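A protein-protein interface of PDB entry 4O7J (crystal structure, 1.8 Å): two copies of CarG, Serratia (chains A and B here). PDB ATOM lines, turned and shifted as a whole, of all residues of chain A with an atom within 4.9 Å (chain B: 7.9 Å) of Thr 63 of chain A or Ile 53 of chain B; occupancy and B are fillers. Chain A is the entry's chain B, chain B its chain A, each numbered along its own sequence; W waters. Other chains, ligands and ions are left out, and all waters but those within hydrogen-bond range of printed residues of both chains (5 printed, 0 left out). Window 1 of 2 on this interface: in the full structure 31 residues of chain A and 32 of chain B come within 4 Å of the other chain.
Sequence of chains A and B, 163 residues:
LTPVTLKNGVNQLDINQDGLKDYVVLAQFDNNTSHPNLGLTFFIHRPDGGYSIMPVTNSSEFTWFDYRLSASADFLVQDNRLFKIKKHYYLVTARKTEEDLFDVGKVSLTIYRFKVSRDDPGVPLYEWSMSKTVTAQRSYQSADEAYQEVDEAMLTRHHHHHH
Water W1 lies within hydrogen-bond range of the side-chain hydroxyl of Ser 52 of chain B (2.6 Å), the backbone carbonyl oxygen of Ile 53 of chain B (2.7 Å) and the backbone carbonyl oxygen of Gln 28 of chain A (3.5 Å).
Water W5 lies within hydrogen-bond range of OG1 of Thr 63 of chain A and OG1 of Thr 63 of chain B.
Water W3 bridges OE2 of Glu 61 of chain A (2.8 Å) and OE2 of Glu 61 of chain B (3.1 Å).
Water W4 lies within hydrogen-bond range of the side-chain carboxylate of Glu 61 of chain A (2.9 Å), the backbone NH of Phe 62 of chain A (2.9 Å), the backbone NH of Phe 62 of chain B (3.1 Å) and the side-chain carboxylate of Glu 61 of chain B (3.2 Å).
Water W2 lies within hydrogen-bond range of the side-chain amide nitrogen of Gln 28 of chain A (2.9 Å) and the guanidinium group of Arg 46 of chain B (3.3 Å).
Printed residues of chain B that touch a printed residue of chain A: Phe 43, Arg 46, Tyr 51, Ser 52, Ile 53, Ser 60, Glu 61 and Phe 62.
Among the printed residues, no Asp or Glu carboxylate lies within 4 Å of a Lys or Arg side-chain nitrogen of the other chain.
NE2 of Gln 28 of chain A sits close to NE of Arg 46 of chain B.
The backbone carbonyl oxygen (O) of Gln 28 of chain A is in hydrogen-bond range of the backbone NH (N) of Ile 53 of chain B, at 2.8 Å.
The side-chain carboxylate (OE2) of Glu 61 of chain A lies close to the backbone carbonyl oxygen (O) of Ser 60 of chain B (2.5 Å).
The backbone carbonyl oxygen of Tyr 51 of chain B lies within hydrogen-bond range of the backbone NH of Gln 28 of chain A (2.8 Å).
Glu 61 of chain A touches Phe 62 of chain B, and with the chains exchanged Phe 62 of chain A touches Glu 61 of chain B.
Positions printed for both chains: 41, 56, 61, 62 and 63.
Of the 13 pairs that touch across the chains among the printed residues, 2 have their exchanged pair printed and touching as well.
O of Glu 61 of chain A sits at hydrogen-bond distance from N of Val 56 of chain A (2.9 Å).
OG1 of Thr 63 of chain A sits at hydrogen-bond distance from OG1 of Thr 41 of chain A.
A ring nitrogen (ND1) of His 45 of chain B sits close to the side-chain hydroxyl (OH) of Tyr 51 of chain B, at 3.4 Å.
The side-chain hydroxyl of Tyr 51 of chain B lies within hydrogen-bond range of the side-chain hydroxyl of Tyr 23 of chain B, 3.4 Å away.
O of Ala 27 of chain A sits at hydrogen-bond distance from N of Gly 39 of chain A (2.8 Å).
The backbone carbonyl oxygen of Tyr 23 of chain B is in hydrogen-bond range of the backbone NH of Phe 43 of chain B (2.8 Å).
Among the printed residues, pairs that only touch across the chains: Ala 27 of chain A with Phe 43 of chain B, Ala 27 of chain A with Tyr 51 of chain B, Gln 28 of chain A with Ser 52 of chain B, Phe 29 of chain A with Ile 53 of chain B, Phe 29 of chain A with Phe 62 of chain B, Glu 61 of chain A with Phe 62 of chain B, Phe 62 of chain A with Glu 61 of chain B, Thr 63 of chain A with Ile 53 of chain B and Phe 65 of chain A with Phe 62 of chain B.
Printed residues of chain B within 4 Å of Thr 63 of chain A: Ile 53.
Of chain A, only Gln 28, Phe 29 and Thr 63 come within 4 Å of Ile 53 of chain B.
Printed residues of chain A within 4 Å of Phe 43 of chain B: Ala 27 (3.6 Å).
Of the printed residues of chain A, Arg 46 of chain B touches Gln 28.
The nearest residue of chain B that does not touch Thr 63 of chain A is Phe 62 of chain B (4.3 Å).
The nearest printed residue of chain A that does not touch Tyr 51 of chain B is Phe 29 of chain A (5.5 Å).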
ATOM      1  N   ALA A  27      26.438 -12.386 -16.162  1.00  0.00           N
ATOM      2  CA  ALA A  27      27.288 -13.084 -15.228  1.00  0.00           C
ATOM      3  C   ALA A  27      28.509 -13.567 -15.952  1.00  0.00           C
ATOM      4  O   ALA A  27      28.629 -13.388 -17.159  1.00  0.00           O
ATOM      5  CB  ALA A  27      26.528 -14.257 -14.616  1.00  0.00           C
ATOM      6  N   GLN A  28      29.430 -14.186 -15.220  1.00  0.00           N
ATOM      7  CA  GLN A  28      30.623 -14.744 -15.809  1.00  0.00           C
ATOM      8  C   GLN A  28      30.874 -16.140 -15.303  1.00  0.00           C
ATOM      9  O   GLN A  28      30.562 -16.457 -14.145  1.00  0.00           O
ATOM     10  CB  GLN A  28      31.791 -13.791 -15.443  1.00  0.00           C
ATOM     11  CG  GLN A  28      32.035 -13.624 -13.957  1.00  0.00           C
ATOM     12  CD  GLN A  28      32.849 -12.382 -13.646  1.00  0.00           C
ATOM     13  OE1 GLN A  28      32.359 -11.274 -13.819  1.00  0.00           O
ATOM     14  NE2 GLN A  28      34.025 -12.551 -13.083  1.00  0.00           N
ATOM     15  N   PHE A  29      31.474 -16.946 -16.131  1.00  0.00           N
ATOM     16  CA  PHE A  29      31.983 -18.248 -15.729  1.00  0.00           C
ATOM     17  C   PHE A  29      33.421 -18.053 -15.395  1.00  0.00           C
ATOM     18  O   PHE A  29      34.216 -17.726 -16.300  1.00  0.00           O
ATOM     19  CB  PHE A  29      31.799 -19.263 -16.836  1.00  0.00           C
ATOM     20  CG  PHE A  29      32.434 -20.567 -16.565  1.00  0.00           C
ATOM     21  CD1 PHE A  29      32.253 -21.193 -15.373  1.00  0.00           C
ATOM     22  CD2 PHE A  29      33.132 -21.240 -17.582  1.00  0.00           C
ATOM     23  CE1 PHE A  29      32.762 -22.454 -15.151  1.00  0.00           C
ATOM     24  CE2 PHE A  29      33.748 -22.426 -17.312  1.00  0.00           C
ATOM     25  CZ  PHE A  29      33.566 -23.058 -16.114  1.00  0.00           C
ATOM     26  N   GLY A  39      28.485 -14.211 -19.802  1.00  0.00           N
ATOM     27  CA  GLY A  39      27.307 -14.886 -20.261  1.00  0.00           C
ATOM     28  C   GLY A  39      26.003 -14.177 -19.943  1.00  0.00           C
ATOM     29  O   GLY A  39      25.881 -13.536 -18.872  1.00  0.00           O
ATOM     30  N   LEU A  40      25.061 -14.239 -20.885  1.00  0.00           N
ATOM     31  CA  LEU A  40      23.715 -13.698 -20.664  1.00  0.00           C
ATOM     32  C   LEU A  40      22.705 -14.873 -20.518  1.00  0.00           C
ATOM     33  O   LEU A  40      22.669 -15.779 -21.375  1.00  0.00           O
ATOM     34  CB  LEU A  40      23.284 -12.921 -21.887  1.00  0.00           C
ATOM     35  CG  LEU A  40      24.176 -11.742 -22.195  1.00  0.00           C
ATOM     36  CD1 LEU A  40      23.736 -11.089 -23.506  1.00  0.00           C
ATOM     37  CD2 LEU A  40      24.104 -10.705 -21.092  1.00  0.00           C
ATOM     38  N   THR A  41      21.867 -14.789 -19.516  1.00  0.00           N
ATOM     39  CA  THR A  41      20.794 -15.769 -19.277  1.00  0.00           C
ATOM     40  C   THR A  41      19.457 -14.977 -19.212  1.00  0.00           C
ATOM     41  O   THR A  41      19.396 -13.931 -18.564  1.00  0.00           O
ATOM     42  CB  THR A  41      21.077 -16.579 -17.980  1.00  0.00           C
ATOM     43  OG1 THR A  41      22.427 -17.075 -17.975  1.00  0.00           O
ATOM     44  CG2 THR A  41      20.112 -17.821 -17.915  1.00  0.00           C
ATOM     45  N   VAL A  56      19.227 -21.237 -25.621  1.00  0.00           N
ATOM     46  CA  VAL A  56      20.160 -20.682 -26.592  1.00  0.00           C
ATOM     47  C   VAL A  56      19.709 -21.319 -27.930  1.00  0.00           C
ATOM     48  O   VAL A  56      19.520 -22.542 -28.014  1.00  0.00           O
ATOM     49  CB  VAL A  56      21.612 -21.038 -26.277  1.00  0.00           C
ATOM     50  CG1 VAL A  56      22.534 -20.617 -27.415  1.00  0.00           C
ATOM     51  CG2 VAL A  56      22.034 -20.338 -24.962  1.00  0.00           C
ATOM     52  N   GLU A  61      22.194 -25.509 -24.603  1.00  0.00           N
ATOM     53  CA  GLU A  61      22.524 -24.589 -23.503  1.00  0.00           C
ATOM     54  C   GLU A  61      21.419 -23.557 -23.218  1.00  0.00           C
ATOM     55  O   GLU A  61      20.555 -23.314 -24.053  1.00  0.00           O
ATOM     56  CB  GLU A  61      23.755 -23.796 -23.871  1.00  0.00           C
ATOM     57  CG  GLU A  61      25.078 -24.559 -23.894  1.00  0.00           C
ATOM     58  CD  GLU A  61      25.841 -24.476 -22.534  1.00  0.00           C
ATOM     59  OE1 GLU A  61      25.565 -23.554 -21.682  1.00  0.00           O
ATOM     60  OE2 GLU A  61      26.743 -25.330 -22.336  1.00  0.00           O
ATOM     61  N   PHE A  62      21.488 -22.929 -22.027  1.00  0.00           N
ATOM     62  CA  PHE A  62      20.550 -21.887 -21.656  1.00  0.00           C
ATOM     63  C   PHE A  62      21.212 -20.558 -21.251  1.00  0.00           C
ATOM     64  O   PHE A  62      20.499 -19.641 -20.871  1.00  0.00           O
ATOM     65  CB  PHE A  62      19.626 -22.362 -20.510  1.00  0.00           C
ATOM     66  CG  PHE A  62      18.589 -23.368 -21.000  1.00  0.00           C
ATOM     67  CD1 PHE A  62      18.965 -24.666 -21.240  1.00  0.00           C
ATOM     68  CD2 PHE A  62      17.334 -22.971 -21.293  1.00  0.00           C
ATOM     69  CE1 PHE A  62      18.036 -25.609 -21.659  1.00  0.00           C
ATOM     70  CE2 PHE A  62      16.390 -23.886 -21.757  1.00  0.00           C
ATOM     71  CZ  PHE A  62      16.759 -25.193 -21.966  1.00  0.00           C
ATOM     72  N   THR A  63      22.537 -20.530 -21.303  1.00  0.00           N
ATOM     73  CA  THR A  63      23.306 -19.251 -21.192  1.00  0.00           C
ATOM     74  C   THR A  63      24.103 -19.008 -22.478  1.00  0.00           C
ATOM     75  O   THR A  63      24.823 -19.909 -22.950  1.00  0.00           O
ATOM     76  CB  THR A  63      24.190 -19.330 -19.930  1.00  0.00           C
ATOM     77  OG1 THR A  63      23.346 -19.565 -18.823  1.00  0.00           O
ATOM     78  CG2 THR A  63      24.997 -18.100 -19.724  1.00  0.00           C
ATOM     79  N   TRP A  64      24.032 -17.772 -22.983  1.00  0.00           N
ATOM     80  CA  TRP A  64      24.790 -17.292 -24.101  1.00  0.00           C
ATOM     81  C   TRP A  64      26.156 -16.778 -23.657  1.00  0.00           C
ATOM     82  O   TRP A  64      26.240 -15.763 -22.992  1.00  0.00           O
ATOM     83  CB  TRP A  64      24.064 -16.145 -24.848  1.00  0.00           C
ATOM     84  CG  TRP A  64      22.720 -16.473 -25.375  1.00  0.00           C
ATOM     85  CD1 TRP A  64      21.578 -16.600 -24.647  1.00  0.00           C
ATOM     86  CD2 TRP A  64      22.351 -16.666 -26.737  1.00  0.00           C
ATOM     87  NE1 TRP A  64      20.534 -16.924 -25.445  1.00  0.00           N
ATOM     88  CE2 TRP A  64      20.976 -17.008 -26.747  1.00  0.00           C
ATOM     89  CE3 TRP A  64      23.058 -16.605 -27.970  1.00  0.00           C
ATOM     90  CZ2 TRP A  64      20.248 -17.164 -27.941  1.00  0.00           C
ATOM     91  CZ3 TRP A  64      22.346 -16.892 -29.152  1.00  0.00           C
ATOM     92  CH2 TRP A  64      20.958 -17.140 -29.135  1.00  0.00           C
ATOM     93  N   PHE A  65      27.228 -17.491 -24.035  1.00  0.00           N
ATOM     94  CA  PHE A  65      28.547 -17.142 -23.609  1.00  0.00           C
ATOM     95  C   PHE A  65      29.361 -16.525 -24.749  1.00  0.00           C
ATOM     96  O   PHE A  65      29.231 -16.926 -25.944  1.00  0.00           O
ATOM     97  CB  PHE A  65      29.290 -18.380 -23.083  1.00  0.00           C
ATOM     98  CG  PHE A  65      28.875 -18.817 -21.711  1.00  0.00           C
ATOM     99  CD1 PHE A  65      29.252 -18.130 -20.590  1.00  0.00           C
ATOM    100  CD2 PHE A  65      28.123 -19.959 -21.575  1.00  0.00           C
ATOM    101  CE1 PHE A  65      28.925 -18.569 -19.337  1.00  0.00           C
ATOM    102  CE2 PHE A  65      27.732 -20.393 -20.309  1.00  0.00           C
ATOM    103  CZ  PHE A  65      28.152 -19.702 -19.205  1.00  0.00           C
ATOM    104  N   TYR B  23      22.453 -15.500  -5.902  1.00  0.00           N
ATOM    105  CA  TYR B  23      21.179 -15.781  -6.538  1.00  0.00           C
ATOM    106  C   TYR B  23      21.066 -17.239  -6.814  1.00  0.00           C
ATOM    107  O   TYR B  23      22.000 -17.908  -7.326  1.00  0.00           O
ATOM    108  CB  TYR B  23      21.068 -15.152  -7.907  1.00  0.00           C
ATOM    109  CG  TYR B  23      21.231 -13.660  -8.083  1.00  0.00           C
ATOM    110  CD1 TYR B  23      20.874 -12.713  -7.120  1.00  0.00           C
ATOM    111  CD2 TYR B  23      21.651 -13.191  -9.350  1.00  0.00           C
ATOM    112  CE1 TYR B  23      21.002 -11.317  -7.423  1.00  0.00           C
ATOM    113  CE2 TYR B  23      21.789 -11.855  -9.633  1.00  0.00           C
ATOM    114  CZ  TYR B  23      21.457 -10.907  -8.685  1.00  0.00           C
ATOM    115  OH  TYR B  23      21.633  -9.557  -9.130  1.00  0.00           O
ATOM    116  N   THR B  41      19.445 -22.217 -11.433  1.00  0.00           N
ATOM    117  CA  THR B  41      20.662 -21.524 -11.935  1.00  0.00           C
ATOM    118  C   THR B  41      21.271 -20.749 -10.784  1.00  0.00           C
ATOM    119  O   THR B  41      20.557 -19.964 -10.134  1.00  0.00           O
ATOM    120  CB  THR B  41      20.316 -20.637 -13.167  1.00  0.00           C
ATOM    121  OG1 THR B  41      19.613 -21.417 -14.143  1.00  0.00           O
ATOM    122  CG2 THR B  41      21.601 -20.218 -13.884  1.00  0.00           C
ATOM    123  N   PHE B  42      22.553 -20.990 -10.507  1.00  0.00           N
ATOM    124  CA  PHE B  42      23.242 -20.428  -9.306  1.00  0.00           C
ATOM    125  C   PHE B  42      24.201 -19.376  -9.756  1.00  0.00           C
ATOM    126  O   PHE B  42      24.992 -19.613 -10.694  1.00  0.00           O
ATOM    127  CB  PHE B  42      24.030 -21.505  -8.582  1.00  0.00           C
ATOM    128  CG  PHE B  42      23.156 -22.541  -7.947  1.00  0.00           C
ATOM    129  CD1 PHE B  42      22.799 -23.645  -8.672  1.00  0.00           C
ATOM    130  CD2 PHE B  42      22.761 -22.413  -6.626  1.00  0.00           C
ATOM    131  CE1 PHE B  42      21.981 -24.620  -8.095  1.00  0.00           C
ATOM    132  CE2 PHE B  42      21.953 -23.390  -6.039  1.00  0.00           C
ATOM    133  CZ  PHE B  42      21.547 -24.452  -6.817  1.00  0.00           C
ATOM    134  N   PHE B  43      24.158 -18.224  -9.105  1.00  0.00           N
ATOM    135  CA  PHE B  43      25.059 -17.136  -9.402  1.00  0.00           C
ATOM    136  C   PHE B  43      25.671 -16.603  -8.064  1.00  0.00           C
ATOM    137  O   PHE B  43      24.915 -16.180  -7.178  1.00  0.00           O
ATOM    138  CB  PHE B  43      24.310 -15.960 -10.001  1.00  0.00           C
ATOM    139  CG  PHE B  43      23.640 -16.233 -11.275  1.00  0.00           C
ATOM    140  CD1 PHE B  43      22.300 -16.666 -11.291  1.00  0.00           C
ATOM    141  CD2 PHE B  43      24.293 -16.005 -12.467  1.00  0.00           C
ATOM    142  CE1 PHE B  43      21.693 -16.952 -12.507  1.00  0.00           C
ATOM    143  CE2 PHE B  43      23.641 -16.280 -13.700  1.00  0.00           C
ATOM    144  CZ  PHE B  43      22.357 -16.748 -13.694  1.00  0.00           C
ATOM    145  N   ILE B  44      26.982 -16.731  -7.912  1.00  0.00           N
ATOM    146  CA  ILE B  44      27.660 -16.363  -6.691  1.00  0.00           C
ATOM    147  C   ILE B  44      28.038 -14.895  -6.836  1.00  0.00           C
ATOM    148  O   ILE B  44      28.647 -14.522  -7.817  1.00  0.00           O
ATOM    149  CB  ILE B  44      28.896 -17.266  -6.421  1.00  0.00           C
ATOM    150  CG1 ILE B  44      28.463 -18.721  -6.233  1.00  0.00           C
ATOM    151  CG2 ILE B  44      29.653 -16.741  -5.242  1.00  0.00           C
ATOM    152  CD1 ILE B  44      27.502 -18.890  -5.079  1.00  0.00           C
ATOM    153  N   HIS B  45      27.697 -14.084  -5.840  1.00  0.00           N
ATOM    154  CA  HIS B  45      27.986 -12.648  -5.848  1.00  0.00           C
ATOM    155  C   HIS B  45      29.484 -12.451  -5.527  1.00  0.00           C
ATOM    156  O   HIS B  45      29.971 -13.038  -4.560  1.00  0.00           O
ATOM    157  CB  HIS B  45      27.114 -11.993  -4.812  1.00  0.00           C
ATOM    158  CG  HIS B  45      27.091 -10.491  -4.880  1.00  0.00           C
ATOM    159  ND1 HIS B  45      26.156  -9.740  -4.207  1.00  0.00           N
ATOM    160  CD2 HIS B  45      27.865  -9.612  -5.555  1.00  0.00           C
ATOM    161  CE1 HIS B  45      26.353  -8.464  -4.463  1.00  0.00           C
ATOM    162  NE2 HIS B  45      27.409  -8.353  -5.247  1.00  0.00           N
ATOM    163  N   ARG B  46      30.242 -11.796  -6.411  1.00  0.00           N
ATOM    164  CA  ARG B  46      31.665 -11.606  -6.164  1.00  0.00           C
ATOM    165  C   ARG B  46      31.889 -10.238  -5.519  1.00  0.00           C
ATOM    166  O   ARG B  46      31.180  -9.313  -5.783  1.00  0.00           O
ATOM    167  CB  ARG B  46      32.482 -11.651  -7.439  1.00  0.00           C
ATOM    168  CG  ARG B  46      32.387 -12.959  -8.234  1.00  0.00           C
ATOM    169  CD  ARG B  46      32.787 -12.727  -9.676  1.00  0.00           C
ATOM    170  NE  ARG B  46      34.099 -12.123  -9.769  1.00  0.00           N
ATOM    171  CZ  ARG B  46      35.262 -12.766  -9.733  1.00  0.00           C
ATOM    172  NH1 ARG B  46      35.316 -14.082  -9.740  1.00  0.00           N
ATOM    173  NH2 ARG B  46      36.386 -12.064  -9.745  1.00  0.00           N
ATOM    174  N   GLY B  50      30.725  -8.492  -9.746  1.00  0.00           N
ATOM    175  CA  GLY B  50      30.368  -9.497 -10.743  1.00  0.00           C
ATOM    176  C   GLY B  50      29.575 -10.642 -10.122  1.00  0.00           C
ATOM    177  O   GLY B  50      29.553 -10.785  -8.879  1.00  0.00           O
ATOM    178  N   TYR B  51      28.872 -11.418 -10.965  1.00  0.00           N
ATOM    179  CA  TYR B  51      28.193 -12.651 -10.479  1.00  0.00           C
ATOM    180  C   TYR B  51      28.768 -13.786 -11.249  1.00  0.00           C
ATOM    181  O   TYR B  51      28.982 -13.684 -12.458  1.00  0.00           O
ATOM    182  CB  TYR B  51      26.681 -12.574 -10.642  1.00  0.00           C
ATOM    183  CG  TYR B  51      25.968 -11.723  -9.655  1.00  0.00           C
ATOM    184  CD1 TYR B  51      25.937 -10.333  -9.822  1.00  0.00           C
ATOM    185  CD2 TYR B  51      25.408 -12.265  -8.528  1.00  0.00           C
ATOM    186  CE1 TYR B  51      25.329  -9.543  -8.925  1.00  0.00           C
ATOM    187  CE2 TYR B  51      24.756 -11.456  -7.608  1.00  0.00           C
ATOM    188  CZ  TYR B  51      24.756 -10.113  -7.799  1.00  0.00           C
ATOM    189  OH  TYR B  51      24.154  -9.247  -6.911  1.00  0.00           O
ATOM    190  N   SER B  52      29.175 -14.796 -10.524  1.00  0.00           N
ATOM    191  CA  SER B  52      29.826 -15.908 -11.062  1.00  0.00           C
ATOM    192  C   SER B  52      28.768 -17.022 -11.214  1.00  0.00           C
ATOM    193  O   SER B  52      28.290 -17.600 -10.230  1.00  0.00           O
ATOM    194  CB  SER B  52      30.935 -16.311 -10.139  1.00  0.00           C
ATOM    195  OG  SER B  52      31.860 -17.262 -10.679  1.00  0.00           O
ATOM    196  N   ILE B  53      28.524 -17.423 -12.441  1.00  0.00           N
ATOM    197  CA  ILE B  53      27.545 -18.498 -12.735  1.00  0.00           C
ATOM    198  C   ILE B  53      28.183 -19.859 -12.517  1.00  0.00           C
ATOM    199  O   ILE B  53      29.275 -20.171 -13.029  1.00  0.00           O
ATOM    200  CB  ILE B  53      26.900 -18.325 -14.146  1.00  0.00           C
ATOM    201  CG1 ILE B  53      25.727 -19.315 -14.361  1.00  0.00           C
ATOM    202  CG2 ILE B  53      27.918 -18.497 -15.241  1.00  0.00           C
ATOM    203  CD1 ILE B  53      24.987 -19.157 -15.674  1.00  0.00           C
ATOM    204  N   MET B  54      27.557 -20.697 -11.723  1.00  0.00           N
ATOM    205  CA  MET B  54      28.071 -22.015 -11.415  1.00  0.00           C
ATOM    206  C   MET B  54      27.703 -23.071 -12.509  1.00  0.00           C
ATOM    207  O   MET B  54      26.572 -23.117 -12.930  1.00  0.00           O
ATOM    208  CB  MET B  54      27.539 -22.499 -10.045  1.00  0.00           C
ATOM    209  CG  MET B  54      27.944 -21.611  -8.875  1.00  0.00           C
ATOM    210  SD  MET B  54      27.287 -22.344  -7.351  1.00  0.00           S
ATOM    211  CE  MET B  54      28.277 -23.783  -7.055  1.00  0.00           C
ATOM    212  N   PRO B  55      28.648 -23.921 -12.902  1.00  0.00           N
ATOM    213  CA  PRO B  55      28.367 -25.015 -13.821  1.00  0.00           C
ATOM    214  C   PRO B  55      27.564 -26.120 -13.139  1.00  0.00           C
ATOM    215  O   PRO B  55      27.528 -26.235 -11.873  1.00  0.00           O
ATOM    216  CB  PRO B  55      29.778 -25.476 -14.262  1.00  0.00           C
ATOM    217  CG  PRO B  55      30.649 -25.167 -13.077  1.00  0.00           C
ATOM    218  CD  PRO B  55      30.083 -23.898 -12.475  1.00  0.00           C
ATOM    219  N   VAL B  56      26.908 -26.918 -13.958  1.00  0.00           N
ATOM    220  CA  VAL B  56      26.360 -28.196 -13.528  1.00  0.00           C
ATOM    221  C   VAL B  56      27.525 -29.202 -13.476  1.00  0.00           C
ATOM    222  O   VAL B  56      28.365 -29.279 -14.424  1.00  0.00           O
ATOM    223  CB  VAL B  56      25.243 -28.664 -14.514  1.00  0.00           C
ATOM    224  CG1 VAL B  56      24.718 -30.072 -14.174  1.00  0.00           C
ATOM    225  CG2 VAL B  56      24.098 -27.668 -14.469  1.00  0.00           C
ATOM    226  N   SER B  60      28.272 -29.688 -19.391  1.00  0.00           N
ATOM    227  CA  SER B  60      28.652 -28.392 -19.963  1.00  0.00           C
ATOM    228  C   SER B  60      27.522 -27.350 -19.748  1.00  0.00           C
ATOM    229  O   SER B  60      27.614 -26.198 -20.204  1.00  0.00           O
ATOM    230  CB  SER B  60      28.953 -28.588 -21.461  1.00  0.00           C
ATOM    231  OG  SER B  60      27.745 -28.834 -22.143  1.00  0.00           O
ATOM    232  N   GLU B  61      26.462 -27.764 -19.114  1.00  0.00           N
ATOM    233  CA  GLU B  61      25.274 -26.919 -18.806  1.00  0.00           C
ATOM    234  C   GLU B  61      25.506 -26.040 -17.547  1.00  0.00           C
ATOM    235  O   GLU B  61      26.370 -26.365 -16.715  1.00  0.00           O
ATOM    236  CB  GLU B  61      24.061 -27.789 -18.475  1.00  0.00           C
ATOM    237  CG  GLU B  61      23.414 -28.540 -19.640  1.00  0.00           C
ATOM    238  CD  GLU B  61      22.215 -27.790 -20.256  1.00  0.00           C
ATOM    239  OE1 GLU B  61      21.688 -26.814 -19.642  1.00  0.00           O
ATOM    240  OE2 GLU B  61      21.787 -28.181 -21.359  1.00  0.00           O
ATOM    241  N   PHE B  62      24.686 -24.982 -17.399  1.00  0.00           N
ATOM    242  CA  PHE B  62      24.752 -24.128 -16.252  1.00  0.00           C
ATOM    243  C   PHE B  62      23.431 -24.008 -15.520  1.00  0.00           C
ATOM    244  O   PHE B  62      23.317 -23.193 -14.564  1.00  0.00           O
ATOM    245  CB  PHE B  62      25.293 -22.718 -16.639  1.00  0.00           C
ATOM    246  CG  PHE B  62      26.762 -22.725 -16.940  1.00  0.00           C
ATOM    247  CD1 PHE B  62      27.217 -23.240 -18.147  1.00  0.00           C
ATOM    248  CD2 PHE B  62      27.657 -22.279 -16.051  1.00  0.00           C
ATOM    249  CE1 PHE B  62      28.563 -23.292 -18.441  1.00  0.00           C
ATOM    250  CE2 PHE B  62      29.007 -22.341 -16.286  1.00  0.00           C
ATOM    251  CZ  PHE B  62      29.463 -22.843 -17.462  1.00  0.00           C
ATOM    252  N   THR B  63      22.441 -24.781 -15.960  1.00  0.00           N
ATOM    253  CA  THR B  63      21.189 -24.909 -15.268  1.00  0.00           C
ATOM    254  C   THR B  63      20.868 -26.377 -14.933  1.00  0.00           C
ATOM    255  O   THR B  63      20.987 -27.254 -15.785  1.00  0.00           O
ATOM    256  CB  THR B  63      20.049 -24.252 -16.119  1.00  0.00           C
ATOM    257  OG1 THR B  63      20.324 -22.862 -16.310  1.00  0.00           O
ATOM    258  CG2 THR B  63      18.687 -24.343 -15.412  1.00  0.00           C
ATOM    259  N   PRO B 124      36.521 -24.866 -12.439  1.00  0.00           N
ATOM    260  CA  PRO B 124      35.589 -23.818 -11.980  1.00  0.00           C
ATOM    261  C   PRO B 124      35.980 -23.248 -10.592  1.00  0.00           C
ATOM    262  O   PRO B 124      36.353 -23.990  -9.674  1.00  0.00           O
ATOM    263  CB  PRO B 124      34.268 -24.571 -11.907  1.00  0.00           C
ATOM    264  CG  PRO B 124      34.435 -25.714 -12.885  1.00  0.00           C
ATOM    265  CD  PRO B 124      35.824 -26.154 -12.730  1.00  0.00           C
ATOM    266  N   LEU B 125      35.853 -21.961 -10.435  1.00  0.00           N
ATOM    267  CA  LEU B 125      36.108 -21.333  -9.186  1.00  0.00           C
ATOM    268  C   LEU B 125      35.093 -21.817  -8.121  1.00  0.00           C
ATOM    269  O   LEU B 125      35.440 -22.123  -6.944  1.00  0.00           O
ATOM    270  CB  LEU B 125      35.963 -19.865  -9.384  1.00  0.00           C
ATOM    271  CG  LEU B 125      36.104 -19.041  -8.085  1.00  0.00           C
ATOM    272  CD1 LEU B 125      37.410 -19.417  -7.395  1.00  0.00           C
ATOM    273  CD2 LEU B 125      36.061 -17.600  -8.500  1.00  0.00           C
ATOM    274  N   TYR B 126      33.831 -21.879  -8.524  1.00  0.00           N
ATOM    275  CA  TYR B 126      32.697 -22.243  -7.612  1.00  0.00           C
ATOM    276  C   TYR B 126      31.933 -23.402  -8.260  1.00  0.00           C
ATOM    277  O   TYR B 126      31.409 -23.291  -9.425  1.00  0.00           O
ATOM    278  CB  TYR B 126      31.732 -21.101  -7.468  1.00  0.00           C
ATOM    279  CG  TYR B 126      32.313 -19.821  -6.909  1.00  0.00           C
ATOM    280  CD1 TYR B 126      32.921 -19.820  -5.651  1.00  0.00           C
ATOM    281  CD2 TYR B 126      32.306 -18.686  -7.613  1.00  0.00           C
ATOM    282  CE1 TYR B 126      33.434 -18.639  -5.117  1.00  0.00           C
ATOM    283  CE2 TYR B 126      32.851 -17.502  -7.102  1.00  0.00           C
ATOM    284  CZ  TYR B 126      33.375 -17.498  -5.811  1.00  0.00           C
ATOM    285  OH  TYR B 126      33.998 -16.370  -5.363  1.00  0.00           O
ATOM    286  N   GLU B 127      31.885 -24.531  -7.578  1.00  0.00           N
ATOM    287  CA  GLU B 127      31.124 -25.673  -8.118  1.00  0.00           C
ATOM    288  C   GLU B 127      30.469 -26.462  -7.020  1.00  0.00           C
ATOM    289  O   GLU B 127      30.686 -26.220  -5.827  1.00  0.00           O
ATOM    290  CB  GLU B 127      32.018 -26.597  -8.946  1.00  0.00           C
ATOM    291  CG  GLU B 127      32.898 -27.366  -8.014  1.00  0.00           C
ATOM    292  CD  GLU B 127      34.070 -28.076  -8.680  1.00  0.00           C
ATOM    293  OE1 GLU B 127      34.220 -28.073  -9.925  1.00  0.00           O
ATOM    294  OE2 GLU B 127      34.785 -28.721  -7.900  1.00  0.00           O
HETATM  295  O   HOH W   1      31.752 -19.200 -12.341  1.00  0.00           O
HETATM  296  O   HOH W   2      35.782 -10.291 -12.439  1.00  0.00           O
HETATM  297  O   HOH W   3      24.605 -27.021 -21.930  1.00  0.00           O
HETATM  298  O   HOH W   4      23.250 -24.070 -19.974  1.00  0.00           O
HETATM  299  O   HOH W   5      22.217 -21.915 -18.201  1.00  0.00           O
